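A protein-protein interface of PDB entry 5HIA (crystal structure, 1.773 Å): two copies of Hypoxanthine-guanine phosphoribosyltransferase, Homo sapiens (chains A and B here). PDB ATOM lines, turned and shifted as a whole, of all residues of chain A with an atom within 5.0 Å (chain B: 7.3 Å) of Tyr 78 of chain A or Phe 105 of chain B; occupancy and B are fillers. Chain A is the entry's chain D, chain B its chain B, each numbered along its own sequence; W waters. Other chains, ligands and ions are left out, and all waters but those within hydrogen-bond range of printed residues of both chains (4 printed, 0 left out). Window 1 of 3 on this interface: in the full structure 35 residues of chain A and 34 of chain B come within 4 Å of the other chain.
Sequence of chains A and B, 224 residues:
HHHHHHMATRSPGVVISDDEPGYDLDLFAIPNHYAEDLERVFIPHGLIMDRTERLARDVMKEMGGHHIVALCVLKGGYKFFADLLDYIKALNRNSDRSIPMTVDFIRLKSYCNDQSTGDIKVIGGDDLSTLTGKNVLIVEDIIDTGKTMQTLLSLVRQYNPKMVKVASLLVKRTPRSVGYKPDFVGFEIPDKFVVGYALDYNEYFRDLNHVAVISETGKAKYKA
Among the printed residues, merely in contact across the chains: Tyr 78 of chain A with Phe 105 of chain B, Leu 74 of chain A with Phe 105 of chain B and Leu 74 of chain A with Leu 74 of chain B.
The side-chain carboxylate (OD1) of Asp 86 of chain B lies within salt-bridge range of the side-chain amino group (NZ) of Lys 79 of chain A (2.7 Å). The backbone carbonyl oxygen (O) of Val 103 of chain B is in hydrogen-bond range of the side-chain amino group (NZ) of Lys 75 of chain A (2.7 Å). NZ of Lys 75 of chain A lies within salt-bridge range of OD1 of Asp 104 of chain B, at 3.5 Å. The side-chain carboxylate (OD2) of Asp 126 of chain B is in salt-bridge range of the side-chain amino group (NZ) of Lys 75 of chain A, 2.6 Å away.
Of chain B, only Phe 105 (3.6 Å) comes within 4 Å of Tyr 78 of chain A. Phe 105 of chain B touches two residues of chain A. Printed residues of chain A within 4 Å of Asp 104 of chain B: Lys 75. Printed residues of chain A within 4 Å of Asp 86 of chain B: Lys 79. Of the printed residues of chain A, Asp 126 of chain B touches Lys 75 (2.6 Å). Of the printed residues of chain B, Lys 75 of chain A touches Val 103 (2.7 Å), Asp 104 (3.2 Å) and Asp 126 (2.6 Å). Printed residues of chain B within 4 Å of Lys 79 of chain A: Asp 86. Ile 106 of chain B touches none of the printed residues of chain A. The nearest residue of chain B that does not touch Tyr 78 of chain A is Leu 85 of chain B (4.1 Å).
Leu 74 of chain A touches its own counterpart, Leu 74 of chain B. Positions printed for both chains: 72, 73, 74, 78, 81 and 82.
Water W3 bridges the side-chain hydroxyl (OH) of Tyr 78 of chain A and the side-chain amino group (NZ) of Lys 89 of chain B. Water W4 bridges the side-chain amino group of Lys 79 of chain A (2.7 Å) and the side-chain carboxylate of Asp 86 of chain B (3.3 Å). Water W1 lies within hydrogen-bond range of the side-chain hydroxyl of Tyr 78 of chain A (2.7 Å), the backbone carbonyl oxygen of Ala 82 of chain B (2.9 Å), the side-chain amino group of Lys 89 of chain B (2.9 Å), the side-chain carboxylate of Asp 86 of chain B (3.0 Å) and the side-chain amino group of Lys 79 of chain A (3.3 Å). Water W2 bridges OH of Tyr 78 of chain B (2.7 Å) and O of Ala 82 of chain A (2.9 Å).
O of Ala 70 of chain B is in hydrogen-bond range of N of Asp 104 of chain B (3.0 Å). The backbone NH of Cys 72 of chain B sits at hydrogen-bond distance from the backbone carbonyl oxygen of Asp 104 of chain B. The backbone carbonyl oxygen of Ile 106 of chain B is in hydrogen-bond range of the backbone NH of Leu 74 of chain B. The side-chain carboxylate (OD1) of Asp 86 of chain B is in salt-bridge range of the side-chain amino group (NZ) of Lys 89 of chain B, at 2.7 Å. The backbone NH (N) of Asp 126 of chain B is in hydrogen-bond range of the side-chain carboxylate (OD2) of Asp 104 of chain B.
Of the 12 printed residues of chain A, 4 touch a printed residue of chain B. Hydrophobic or aromatic side chains of chain A that line the printed part of chain B: Leu 74 and Tyr 78.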
ATOM      1  N   CYS A  72       0.006  -0.756  -2.972  1.00  0.00           N
ATOM      2  CA  CYS A  72      -0.219  -1.665  -1.858  1.00  0.00           C
ATOM      3  C   CYS A  72       1.086  -2.023  -1.138  1.00  0.00           C
ATOM      4  O   CYS A  72       2.042  -2.486  -1.771  1.00  0.00           O
ATOM      5  CB  CYS A  72      -0.904  -2.934  -2.361  1.00  0.00           C
ATOM      6  SG  CYS A  72      -1.207  -4.192  -1.105  1.00  0.00           S
ATOM      7  N   VAL A  73       1.136  -1.817   0.182  1.00  0.00           N
ATOM      8  CA  VAL A  73       2.302  -2.246   0.959  1.00  0.00           C
ATOM      9  C   VAL A  73       2.059  -3.677   1.463  1.00  0.00           C
ATOM     10  O   VAL A  73       1.322  -3.905   2.445  1.00  0.00           O
ATOM     11  CB  VAL A  73       2.623  -1.298   2.169  1.00  0.00           C
ATOM     12  CG1 VAL A  73       3.934  -1.700   2.836  1.00  0.00           C
ATOM     13  CG2 VAL A  73       2.719   0.153   1.717  1.00  0.00           C
ATOM     14  N   LEU A  74       2.661  -4.633   0.761  1.00  0.00           N
ATOM     15  CA  LEU A  74       2.585  -6.056   1.093  1.00  0.00           C
ATOM     16  C   LEU A  74       3.366  -6.372   2.365  1.00  0.00           C
ATOM     17  O   LEU A  74       4.266  -5.617   2.725  1.00  0.00           O
ATOM     18  CB  LEU A  74       3.140  -6.893  -0.070  1.00  0.00           C
ATOM     19  CG  LEU A  74       2.295  -6.797  -1.339  1.00  0.00           C
ATOM     20  CD1 LEU A  74       3.002  -7.445  -2.527  1.00  0.00           C
ATOM     21  CD2 LEU A  74       0.941  -7.445  -1.082  1.00  0.00           C
ATOM     22  N   LYS A  75       3.047  -7.474   3.048  1.00  0.00           N
ATOM     23  CA  LYS A  75       1.899  -8.332   2.740  1.00  0.00           C
ATOM     24  C   LYS A  75       0.644  -7.856   3.452  1.00  0.00           C
ATOM     25  O   LYS A  75      -0.464  -8.042   2.958  1.00  0.00           O
ATOM     26  CB  LYS A  75       2.166  -9.785   3.153  1.00  0.00           C
ATOM     27  CG  LYS A  75       3.379 -10.467   2.507  1.00  0.00           C
ATOM     28  CD  LYS A  75       3.443 -11.894   3.037  1.00  0.00           C
ATOM     29  CE  LYS A  75       4.714 -12.624   2.631  1.00  0.00           C
ATOM     30  NZ  LYS A  75       4.671 -14.047   3.115  1.00  0.00           N
ATOM     31  N   GLY A  76       0.828  -7.248   4.623  1.00  0.00           N
ATOM     32  CA  GLY A  76      -0.286  -6.862   5.486  1.00  0.00           C
ATOM     33  C   GLY A  76      -1.351  -6.007   4.826  1.00  0.00           C
ATOM     34  O   GLY A  76      -2.528  -6.089   5.173  1.00  0.00           O
ATOM     35  N   GLY A  77      -0.948  -5.205   3.843  1.00  0.00           N
ATOM     36  CA  GLY A  77      -1.862  -4.259   3.239  1.00  0.00           C
ATOM     37  C   GLY A  77      -2.835  -4.859   2.239  1.00  0.00           C
ATOM     38  O   GLY A  77      -3.773  -4.176   1.827  1.00  0.00           O
ATOM     39  N   TYR A  78      -2.647  -6.130   1.875  1.00  0.00           N
ATOM     40  CA  TYR A  78      -3.317  -6.685   0.695  1.00  0.00           C
ATOM     41  C   TYR A  78      -4.854  -6.752   0.814  1.00  0.00           C
ATOM     42  O   TYR A  78      -5.548  -6.466  -0.162  1.00  0.00           O
ATOM     43  CB  TYR A  78      -2.726  -8.065   0.358  1.00  0.00           C
ATOM     44  CG  TYR A  78      -3.596  -9.271   0.637  1.00  0.00           C
ATOM     45  CD1 TYR A  78      -4.581  -9.674  -0.265  1.00  0.00           C
ATOM     46  CD2 TYR A  78      -3.416 -10.031   1.788  1.00  0.00           C
ATOM     47  CE1 TYR A  78      -5.380 -10.769  -0.008  1.00  0.00           C
ATOM     48  CE2 TYR A  78      -4.206 -11.146   2.046  1.00  0.00           C
ATOM     49  CZ  TYR A  78      -5.184 -11.508   1.140  1.00  0.00           C
ATOM     50  OH  TYR A  78      -5.973 -12.610   1.386  1.00  0.00           O
ATOM     51  N   LYS A  79      -5.396  -7.123   1.972  1.00  0.00           N
ATOM     52  CA  LYS A  79      -6.863  -7.211   2.097  1.00  0.00           C
ATOM     53  C   LYS A  79      -7.532  -5.836   2.081  1.00  0.00           C
ATOM     54  O   LYS A  79      -8.492  -5.611   1.324  1.00  0.00           O
ATOM     55  CB  LYS A  79      -7.283  -7.959   3.369  1.00  0.00           C
ATOM     56  CG  LYS A  79      -7.402  -9.459   3.213  1.00  0.00           C
ATOM     57  CD  LYS A  79      -8.246  -9.839   2.009  1.00  0.00           C
ATOM     58  CE  LYS A  79      -9.715  -9.769   2.317  1.00  0.00           C
ATOM     59  NZ  LYS A  79     -10.527 -10.132   1.123  1.00  0.00           N
ATOM     60  N   PHE A  80      -7.039  -4.935   2.930  1.00  0.00           N
ATOM     61  CA  PHE A  80      -7.513  -3.556   2.972  1.00  0.00           C
ATOM     62  C   PHE A  80      -7.433  -2.910   1.587  1.00  0.00           C
ATOM     63  O   PHE A  80      -8.374  -2.239   1.135  1.00  0.00           O
ATOM     64  CB  PHE A  80      -6.705  -2.748   4.009  1.00  0.00           C
ATOM     65  CG  PHE A  80      -7.213  -1.349   4.223  1.00  0.00           C
ATOM     66  CD1 PHE A  80      -8.568  -1.108   4.453  1.00  0.00           C
ATOM     67  CD2 PHE A  80      -6.340  -0.275   4.199  1.00  0.00           C
ATOM     68  CE1 PHE A  80      -9.030   0.179   4.645  1.00  0.00           C
ATOM     69  CE2 PHE A  80      -6.787   1.006   4.391  1.00  0.00           C
ATOM     70  CZ  PHE A  80      -8.145   1.238   4.619  1.00  0.00           C
ATOM     71  N   PHE A  81      -6.313  -3.153   0.904  1.00  0.00           N
ATOM     72  CA  PHE A  81      -6.099  -2.663  -0.455  1.00  0.00           C
ATOM     73  C   PHE A  81      -7.182  -3.178  -1.403  1.00  0.00           C
ATOM     74  O   PHE A  81      -7.826  -2.388  -2.105  1.00  0.00           O
ATOM     75  CB  PHE A  81      -4.703  -3.084  -0.939  1.00  0.00           C
ATOM     76  CG  PHE A  81      -4.365  -2.654  -2.347  1.00  0.00           C
ATOM     77  CD1 PHE A  81      -3.962  -1.353  -2.616  1.00  0.00           C
ATOM     78  CD2 PHE A  81      -4.408  -3.556  -3.392  1.00  0.00           C
ATOM     79  CE1 PHE A  81      -3.625  -0.961  -3.903  1.00  0.00           C
ATOM     80  CE2 PHE A  81      -4.071  -3.164  -4.692  1.00  0.00           C
ATOM     81  CZ  PHE A  81      -3.672  -1.867  -4.940  1.00  0.00           C
ATOM     82  N   ALA A  82      -7.384  -4.493  -1.429  1.00  0.00           N
ATOM     83  CA  ALA A  82      -8.356  -5.070  -2.357  1.00  0.00           C
ATOM     84  C   ALA A  82      -9.755  -4.534  -2.069  1.00  0.00           C
ATOM     85  O   ALA A  82     -10.493  -4.179  -2.986  1.00  0.00           O
ATOM     86  CB  ALA A  82      -8.336  -6.595  -2.287  1.00  0.00           C
ATOM     87  N   ALA A 198      -5.442 -10.027   7.111  1.00  0.00           N
ATOM     88  CA  ALA A 198      -4.102 -10.002   6.504  1.00  0.00           C
ATOM     89  C   ALA A 198      -2.990  -9.541   7.464  1.00  0.00           C
ATOM     90  O   ALA A 198      -1.813  -9.602   7.108  1.00  0.00           O
ATOM     91  CB  ALA A 198      -4.090  -9.150   5.217  1.00  0.00           C
ATOM     92  N   ALA B  70      -0.393 -20.212  -0.329  1.00  0.00           N
ATOM     93  CA  ALA B  70      -1.003 -19.674  -1.529  1.00  0.00           C
ATOM     94  C   ALA B  70      -0.083 -18.610  -2.102  1.00  0.00           C
ATOM     95  O   ALA B  70       0.259 -17.642  -1.410  1.00  0.00           O
ATOM     96  CB  ALA B  70      -2.359 -19.106  -1.216  1.00  0.00           C
ATOM     97  N   LEU B  71       0.347 -18.822  -3.341  1.00  0.00           N
ATOM     98  CA  LEU B  71       1.250 -17.891  -4.009  1.00  0.00           C
ATOM     99  C   LEU B  71       0.515 -17.091  -5.065  1.00  0.00           C
ATOM    100  O   LEU B  71      -0.010 -17.649  -6.006  1.00  0.00           O
ATOM    101  CB  LEU B  71       2.419 -18.624  -4.668  1.00  0.00           C
ATOM    102  CG  LEU B  71       3.333 -19.469  -3.785  1.00  0.00           C
ATOM    103  CD1 LEU B  71       4.456 -20.063  -4.618  1.00  0.00           C
ATOM    104  CD2 LEU B  71       3.912 -18.632  -2.666  1.00  0.00           C
ATOM    105  N   CYS B  72       0.485 -15.776  -4.890  1.00  0.00           N
ATOM    106  CA  CYS B  72      -0.164 -14.885  -5.850  1.00  0.00           C
ATOM    107  C   CYS B  72       0.817 -14.378  -6.904  1.00  0.00           C
ATOM    108  O   CYS B  72       1.823 -13.746  -6.573  1.00  0.00           O
ATOM    109  CB  CYS B  72      -0.782 -13.694  -5.117  1.00  0.00           C
ATOM    110  SG  CYS B  72      -1.581 -12.473  -6.192  1.00  0.00           S
ATOM    111  N   VAL B  73       0.533 -14.644  -8.175  1.00  0.00           N
ATOM    112  CA  VAL B  73       1.352 -14.089  -9.232  1.00  0.00           C
ATOM    113  C   VAL B  73       0.876 -12.697  -9.626  1.00  0.00           C
ATOM    114  O   VAL B  73      -0.102 -12.540 -10.377  1.00  0.00           O
ATOM    115  CB  VAL B  73       1.376 -15.012 -10.470  1.00  0.00           C
ATOM    116  CG1 VAL B  73       2.364 -14.498 -11.498  1.00  0.00           C
ATOM    117  CG2 VAL B  73       1.748 -16.440 -10.045  1.00  0.00           C
ATOM    118  N   LEU B  74       1.608 -11.690  -9.139  1.00  0.00           N
ATOM    119  CA  LEU B  74       1.336 -10.278  -9.409  1.00  0.00           C
ATOM    120  C   LEU B  74       1.671  -9.909 -10.851  1.00  0.00           C
ATOM    121  O   LEU B  74       2.465 -10.609 -11.486  1.00  0.00           O
ATOM    122  CB  LEU B  74       2.135  -9.403  -8.442  1.00  0.00           C
ATOM    123  CG  LEU B  74       1.789  -9.600  -6.969  1.00  0.00           C
ATOM    124  CD1 LEU B  74       2.759  -8.810  -6.075  1.00  0.00           C
ATOM    125  CD2 LEU B  74       0.351  -9.172  -6.741  1.00  0.00           C
ATOM    126  N   TYR B  78      -3.935 -10.649  -8.632  1.00  0.00           N
ATOM    127  CA  TYR B  78      -4.289 -10.168  -7.294  1.00  0.00           C
ATOM    128  C   TYR B  78      -5.796 -10.247  -7.000  1.00  0.00           C
ATOM    129  O   TYR B  78      -6.171 -10.600  -5.888  1.00  0.00           O
ATOM    130  CB  TYR B  78      -3.762  -8.742  -7.069  1.00  0.00           C
ATOM    131  CG  TYR B  78      -4.772  -7.605  -7.146  1.00  0.00           C
ATOM    132  CD1 TYR B  78      -5.552  -7.259  -6.041  1.00  0.00           C
ATOM    133  CD2 TYR B  78      -4.913  -6.847  -8.308  1.00  0.00           C
ATOM    134  CE1 TYR B  78      -6.471  -6.215  -6.106  1.00  0.00           C
ATOM    135  CE2 TYR B  78      -5.816  -5.786  -8.377  1.00  0.00           C
ATOM    136  CZ  TYR B  78      -6.600  -5.478  -7.268  1.00  0.00           C
ATOM    137  OH  TYR B  78      -7.508  -4.431  -7.327  1.00  0.00           O
ATOM    138  N   PHE B  81      -6.891 -13.942  -6.802  1.00  0.00           N
ATOM    139  CA  PHE B  81      -6.313 -14.426  -5.558  1.00  0.00           C
ATOM    140  C   PHE B  81      -7.151 -14.006  -4.345  1.00  0.00           C
ATOM    141  O   PHE B  81      -7.513 -14.840  -3.493  1.00  0.00           O
ATOM    142  CB  PHE B  81      -4.872 -13.899  -5.454  1.00  0.00           C
ATOM    143  CG  PHE B  81      -4.115 -14.374  -4.249  1.00  0.00           C
ATOM    144  CD1 PHE B  81      -3.473 -15.607  -4.267  1.00  0.00           C
ATOM    145  CD2 PHE B  81      -3.978 -13.560  -3.129  1.00  0.00           C
ATOM    146  CE1 PHE B  81      -2.711 -16.031  -3.171  1.00  0.00           C
ATOM    147  CE2 PHE B  81      -3.240 -13.976  -2.033  1.00  0.00           C
ATOM    148  CZ  PHE B  81      -2.593 -15.211  -2.052  1.00  0.00           C
ATOM    149  N   ALA B  82      -7.463 -12.717  -4.262  1.00  0.00           N
ATOM    150  CA  ALA B  82      -8.183 -12.218  -3.088  1.00  0.00           C
ATOM    151  C   ALA B  82      -9.561 -12.879  -2.970  1.00  0.00           C
ATOM    152  O   ALA B  82      -9.984 -13.280  -1.875  1.00  0.00           O
ATOM    153  CB  ALA B  82      -8.310 -10.706  -3.153  1.00  0.00           C
ATOM    154  N   ASP B  83     -10.242 -13.024  -4.104  1.00  0.00           N
ATOM    155  CA  ASP B  83     -11.608 -13.530  -4.094  1.00  0.00           C
ATOM    156  C   ASP B  83     -11.621 -15.042  -3.826  1.00  0.00           C
ATOM    157  O   ASP B  83     -12.451 -15.536  -3.040  1.00  0.00           O
ATOM    158  CB  ASP B  83     -12.321 -13.203  -5.413  1.00  0.00           C
ATOM    159  CG  ASP B  83     -12.664 -11.732  -5.548  1.00  0.00           C
ATOM    160  OD1 ASP B  83     -12.837 -11.070  -4.504  1.00  0.00           O
ATOM    161  OD2 ASP B  83     -12.816 -11.242  -6.696  1.00  0.00           O
ATOM    162  N   LEU B  85      -9.390 -16.783  -2.183  1.00  0.00           N
ATOM    163  CA  LEU B  85      -9.071 -16.960  -0.784  1.00  0.00           C
ATOM    164  C   LEU B  85     -10.223 -16.521   0.125  1.00  0.00           C
ATOM    165  O   LEU B  85     -10.396 -17.086   1.196  1.00  0.00           O
ATOM    166  CB  LEU B  85      -7.785 -16.201  -0.453  1.00  0.00           C
ATOM    167  CG  LEU B  85      -6.530 -17.072  -0.582  1.00  0.00           C
ATOM    168  CD1 LEU B  85      -6.306 -17.643  -1.973  1.00  0.00           C
ATOM    169  CD2 LEU B  85      -5.288 -16.325  -0.091  1.00  0.00           C
ATOM    170  N   ASP B  86     -11.006 -15.524  -0.291  1.00  0.00           N
ATOM    171  CA  ASP B  86     -12.175 -15.138   0.498  1.00  0.00           C
ATOM    172  C   ASP B  86     -13.174 -16.286   0.534  1.00  0.00           C
ATOM    173  O   ASP B  86     -13.750 -16.564   1.579  1.00  0.00           O
ATOM    174  CB  ASP B  86     -12.848 -13.877  -0.046  1.00  0.00           C
ATOM    175  CG  ASP B  86     -12.237 -12.613   0.491  1.00  0.00           C
ATOM    176  OD1 ASP B  86     -11.421 -12.699   1.441  1.00  0.00           O
ATOM    177  OD2 ASP B  86     -12.606 -11.523  -0.004  1.00  0.00           O
ATOM    178  N   LYS B  89     -11.747 -18.946   2.750  1.00  0.00           N
ATOM    179  CA  LYS B  89     -11.944 -18.540   4.157  1.00  0.00           C
ATOM    180  C   LYS B  89     -13.375 -18.820   4.598  1.00  0.00           C
ATOM    181  O   LYS B  89     -13.619 -19.256   5.730  1.00  0.00           O
ATOM    182  CB  LYS B  89     -11.618 -17.057   4.367  1.00  0.00           C
ATOM    183  CG  LYS B  89     -10.117 -16.726   4.349  1.00  0.00           C
ATOM    184  CD  LYS B  89      -9.831 -15.392   5.042  1.00  0.00           C
ATOM    185  CE  LYS B  89     -10.308 -14.191   4.240  1.00  0.00           C
ATOM    186  NZ  LYS B  89      -9.611 -14.060   2.937  1.00  0.00           N
ATOM    187  N   VAL B 103       0.377 -16.916   2.955  1.00  0.00           N
ATOM    188  CA  VAL B 103       0.356 -16.328   1.624  1.00  0.00           C
ATOM    189  C   VAL B 103       1.683 -15.684   1.258  1.00  0.00           C
ATOM    190  O   VAL B 103       2.490 -15.323   2.127  1.00  0.00           O
ATOM    191  CB  VAL B 103      -0.784 -15.252   1.463  1.00  0.00           C
ATOM    192  CG1 VAL B 103      -2.169 -15.867   1.666  1.00  0.00           C
ATOM    193  CG2 VAL B 103      -0.559 -14.083   2.391  1.00  0.00           C
ATOM    194  N   ASP B 104       1.925 -15.583  -0.043  1.00  0.00           N
ATOM    195  CA  ASP B 104       3.083 -14.853  -0.541  1.00  0.00           C
ATOM    196  C   ASP B 104       2.732 -14.289  -1.912  1.00  0.00           C
ATOM    197  O   ASP B 104       1.803 -14.762  -2.566  1.00  0.00           O
ATOM    198  CB  ASP B 104       4.303 -15.752  -0.597  1.00  0.00           C
ATOM    199  CG  ASP B 104       5.609 -14.971  -0.572  1.00  0.00           C
ATOM    200  OD1 ASP B 104       5.596 -13.761  -0.254  1.00  0.00           O
ATOM    201  OD2 ASP B 104       6.656 -15.583  -0.864  1.00  0.00           O
ATOM    202  N   PHE B 105       3.444 -13.246  -2.316  1.00  0.00           N
ATOM    203  CA  PHE B 105       3.148 -12.534  -3.545  1.00  0.00           C
ATOM    204  C   PHE B 105       4.439 -12.464  -4.315  1.00  0.00           C
ATOM    205  O   PHE B 105       5.475 -12.103  -3.746  1.00  0.00           O
ATOM    206  CB  PHE B 105       2.598 -11.133  -3.252  1.00  0.00           C
ATOM    207  CG  PHE B 105       1.369 -11.137  -2.382  1.00  0.00           C
ATOM    208  CD1 PHE B 105       1.472 -11.285  -0.997  1.00  0.00           C
ATOM    209  CD2 PHE B 105       0.109 -11.009  -2.946  1.00  0.00           C
ATOM    210  CE1 PHE B 105       0.331 -11.295  -0.198  1.00  0.00           C
ATOM    211  CE2 PHE B 105      -1.021 -11.016  -2.159  1.00  0.00           C
ATOM    212  CZ  PHE B 105      -0.912 -11.155  -0.779  1.00  0.00           C
ATOM    213  N   ILE B 106       4.410 -12.847  -5.586  1.00  0.00           N
ATOM    214  CA  ILE B 106       5.646 -12.834  -6.360  1.00  0.00           C
ATOM    215  C   ILE B 106       5.429 -12.138  -7.685  1.00  0.00           C
ATOM    216  O   ILE B 106       4.337 -12.198  -8.258  1.00  0.00           O
ATOM    217  CB  ILE B 106       6.178 -14.248  -6.617  1.00  0.00           C
ATOM    218  CG1 ILE B 106       5.117 -15.102  -7.310  1.00  0.00           C
ATOM    219  CG2 ILE B 106       6.624 -14.890  -5.314  1.00  0.00           C
ATOM    220  CD1 ILE B 106       5.603 -16.466  -7.735  1.00  0.00           C
ATOM    221  N   ARG B 107       6.472 -11.462  -8.156  1.00  0.00           N
ATOM    222  CA  ARG B 107       6.444 -10.866  -9.476  1.00  0.00           C
ATOM    223  C   ARG B 107       7.496 -11.569 -10.299  1.00  0.00           C
ATOM    224  O   ARG B 107       8.527 -11.969  -9.767  1.00  0.00           O
ATOM    225  CB  ARG B 107       6.694  -9.358  -9.418  1.00  0.00           C
ATOM    226  CG  ARG B 107       5.455  -8.557  -9.795  1.00  0.00           C
ATOM    227  CD  ARG B 107       5.684  -7.059  -9.726  1.00  0.00           C
ATOM    228  NE  ARG B 107       5.702  -6.454 -11.052  1.00  0.00           N
ATOM    229  CZ  ARG B 107       5.650  -5.143 -11.267  1.00  0.00           C
ATOM    230  NH1 ARG B 107       5.563  -4.311 -10.241  1.00  0.00           N
ATOM    231  NH2 ARG B 107       5.675  -4.669 -12.504  1.00  0.00           N
ATOM    232  N   VAL B 122      12.347 -14.475  -9.730  1.00  0.00           N
ATOM    233  CA  VAL B 122      11.220 -14.293  -8.830  1.00  0.00           C
ATOM    234  C   VAL B 122      11.499 -13.143  -7.868  1.00  0.00           C
ATOM    235  O   VAL B 122      12.459 -13.187  -7.090  1.00  0.00           O
ATOM    236  CB  VAL B 122      10.939 -15.578  -8.045  1.00  0.00           C
ATOM    237  CG1 VAL B 122       9.875 -15.331  -6.966  1.00  0.00           C
ATOM    238  CG2 VAL B 122      10.526 -16.683  -9.007  1.00  0.00           C
ATOM    239  N   ILE B 123      10.664 -12.111  -7.926  1.00  0.00           N
ATOM    240  CA  ILE B 123      10.889 -10.897  -7.148  1.00  0.00           C
ATOM    241  C   ILE B 123       9.850 -10.693  -6.039  1.00  0.00           C
ATOM    242  O   ILE B 123       8.641 -10.787  -6.278  1.00  0.00           O
ATOM    243  CB  ILE B 123      10.901  -9.665  -8.074  1.00  0.00           C
ATOM    244  CG1 ILE B 123      12.110  -9.731  -9.017  1.00  0.00           C
ATOM    245  CG2 ILE B 123      10.903  -8.375  -7.262  1.00  0.00           C
ATOM    246  CD1 ILE B 123      12.095  -8.696 -10.118  1.00  0.00           C
ATOM    247  N   GLY B 124      10.329 -10.442  -4.820  1.00  0.00           N
ATOM    248  CA  GLY B 124       9.462 -10.006  -3.735  1.00  0.00           C
ATOM    249  C   GLY B 124       8.846 -11.077  -2.848  1.00  0.00           C
ATOM    250  O   GLY B 124       8.041 -10.771  -1.950  1.00  0.00           O
ATOM    251  N   GLY B 125       9.218 -12.332  -3.079  1.00  0.00           N
ATOM    252  CA  GLY B 125       8.665 -13.426  -2.303  1.00  0.00           C
ATOM    253  C   GLY B 125       9.503 -13.760  -1.080  1.00  0.00           C
ATOM    254  O   GLY B 125      10.573 -13.190  -0.874  1.00  0.00           O
ATOM    255  N   ASP B 126       9.007 -14.687  -0.266  1.00  0.00           N
ATOM    256  CA  ASP B 126       9.785 -15.242   0.834  1.00  0.00           C
ATOM    257  C   ASP B 126      10.793 -16.226   0.278  1.00  0.00           C
ATOM    258  O   ASP B 126      10.696 -16.625  -0.888  1.00  0.00           O
ATOM    259  CB  ASP B 126       8.882 -15.938   1.853  1.00  0.00           C
ATOM    260  CG  ASP B 126       7.889 -14.992   2.499  1.00  0.00           C
ATOM    261  OD1 ASP B 126       8.198 -13.788   2.609  1.00  0.00           O
ATOM    262  OD2 ASP B 126       6.804 -15.460   2.902  1.00  0.00           O
HETATM  263  O   HOH W   1      -8.547 -12.732   0.538  1.00  0.00           O
HETATM  264  O   HOH W   2      -9.728  -4.486  -5.715  1.00  0.00           O
HETATM  265  O   HOH W   3      -6.469 -14.462   2.906  1.00  0.00           O
HETATM  266  O   HOH W   4     -11.340  -8.626  -0.941  1.00  0.00           O
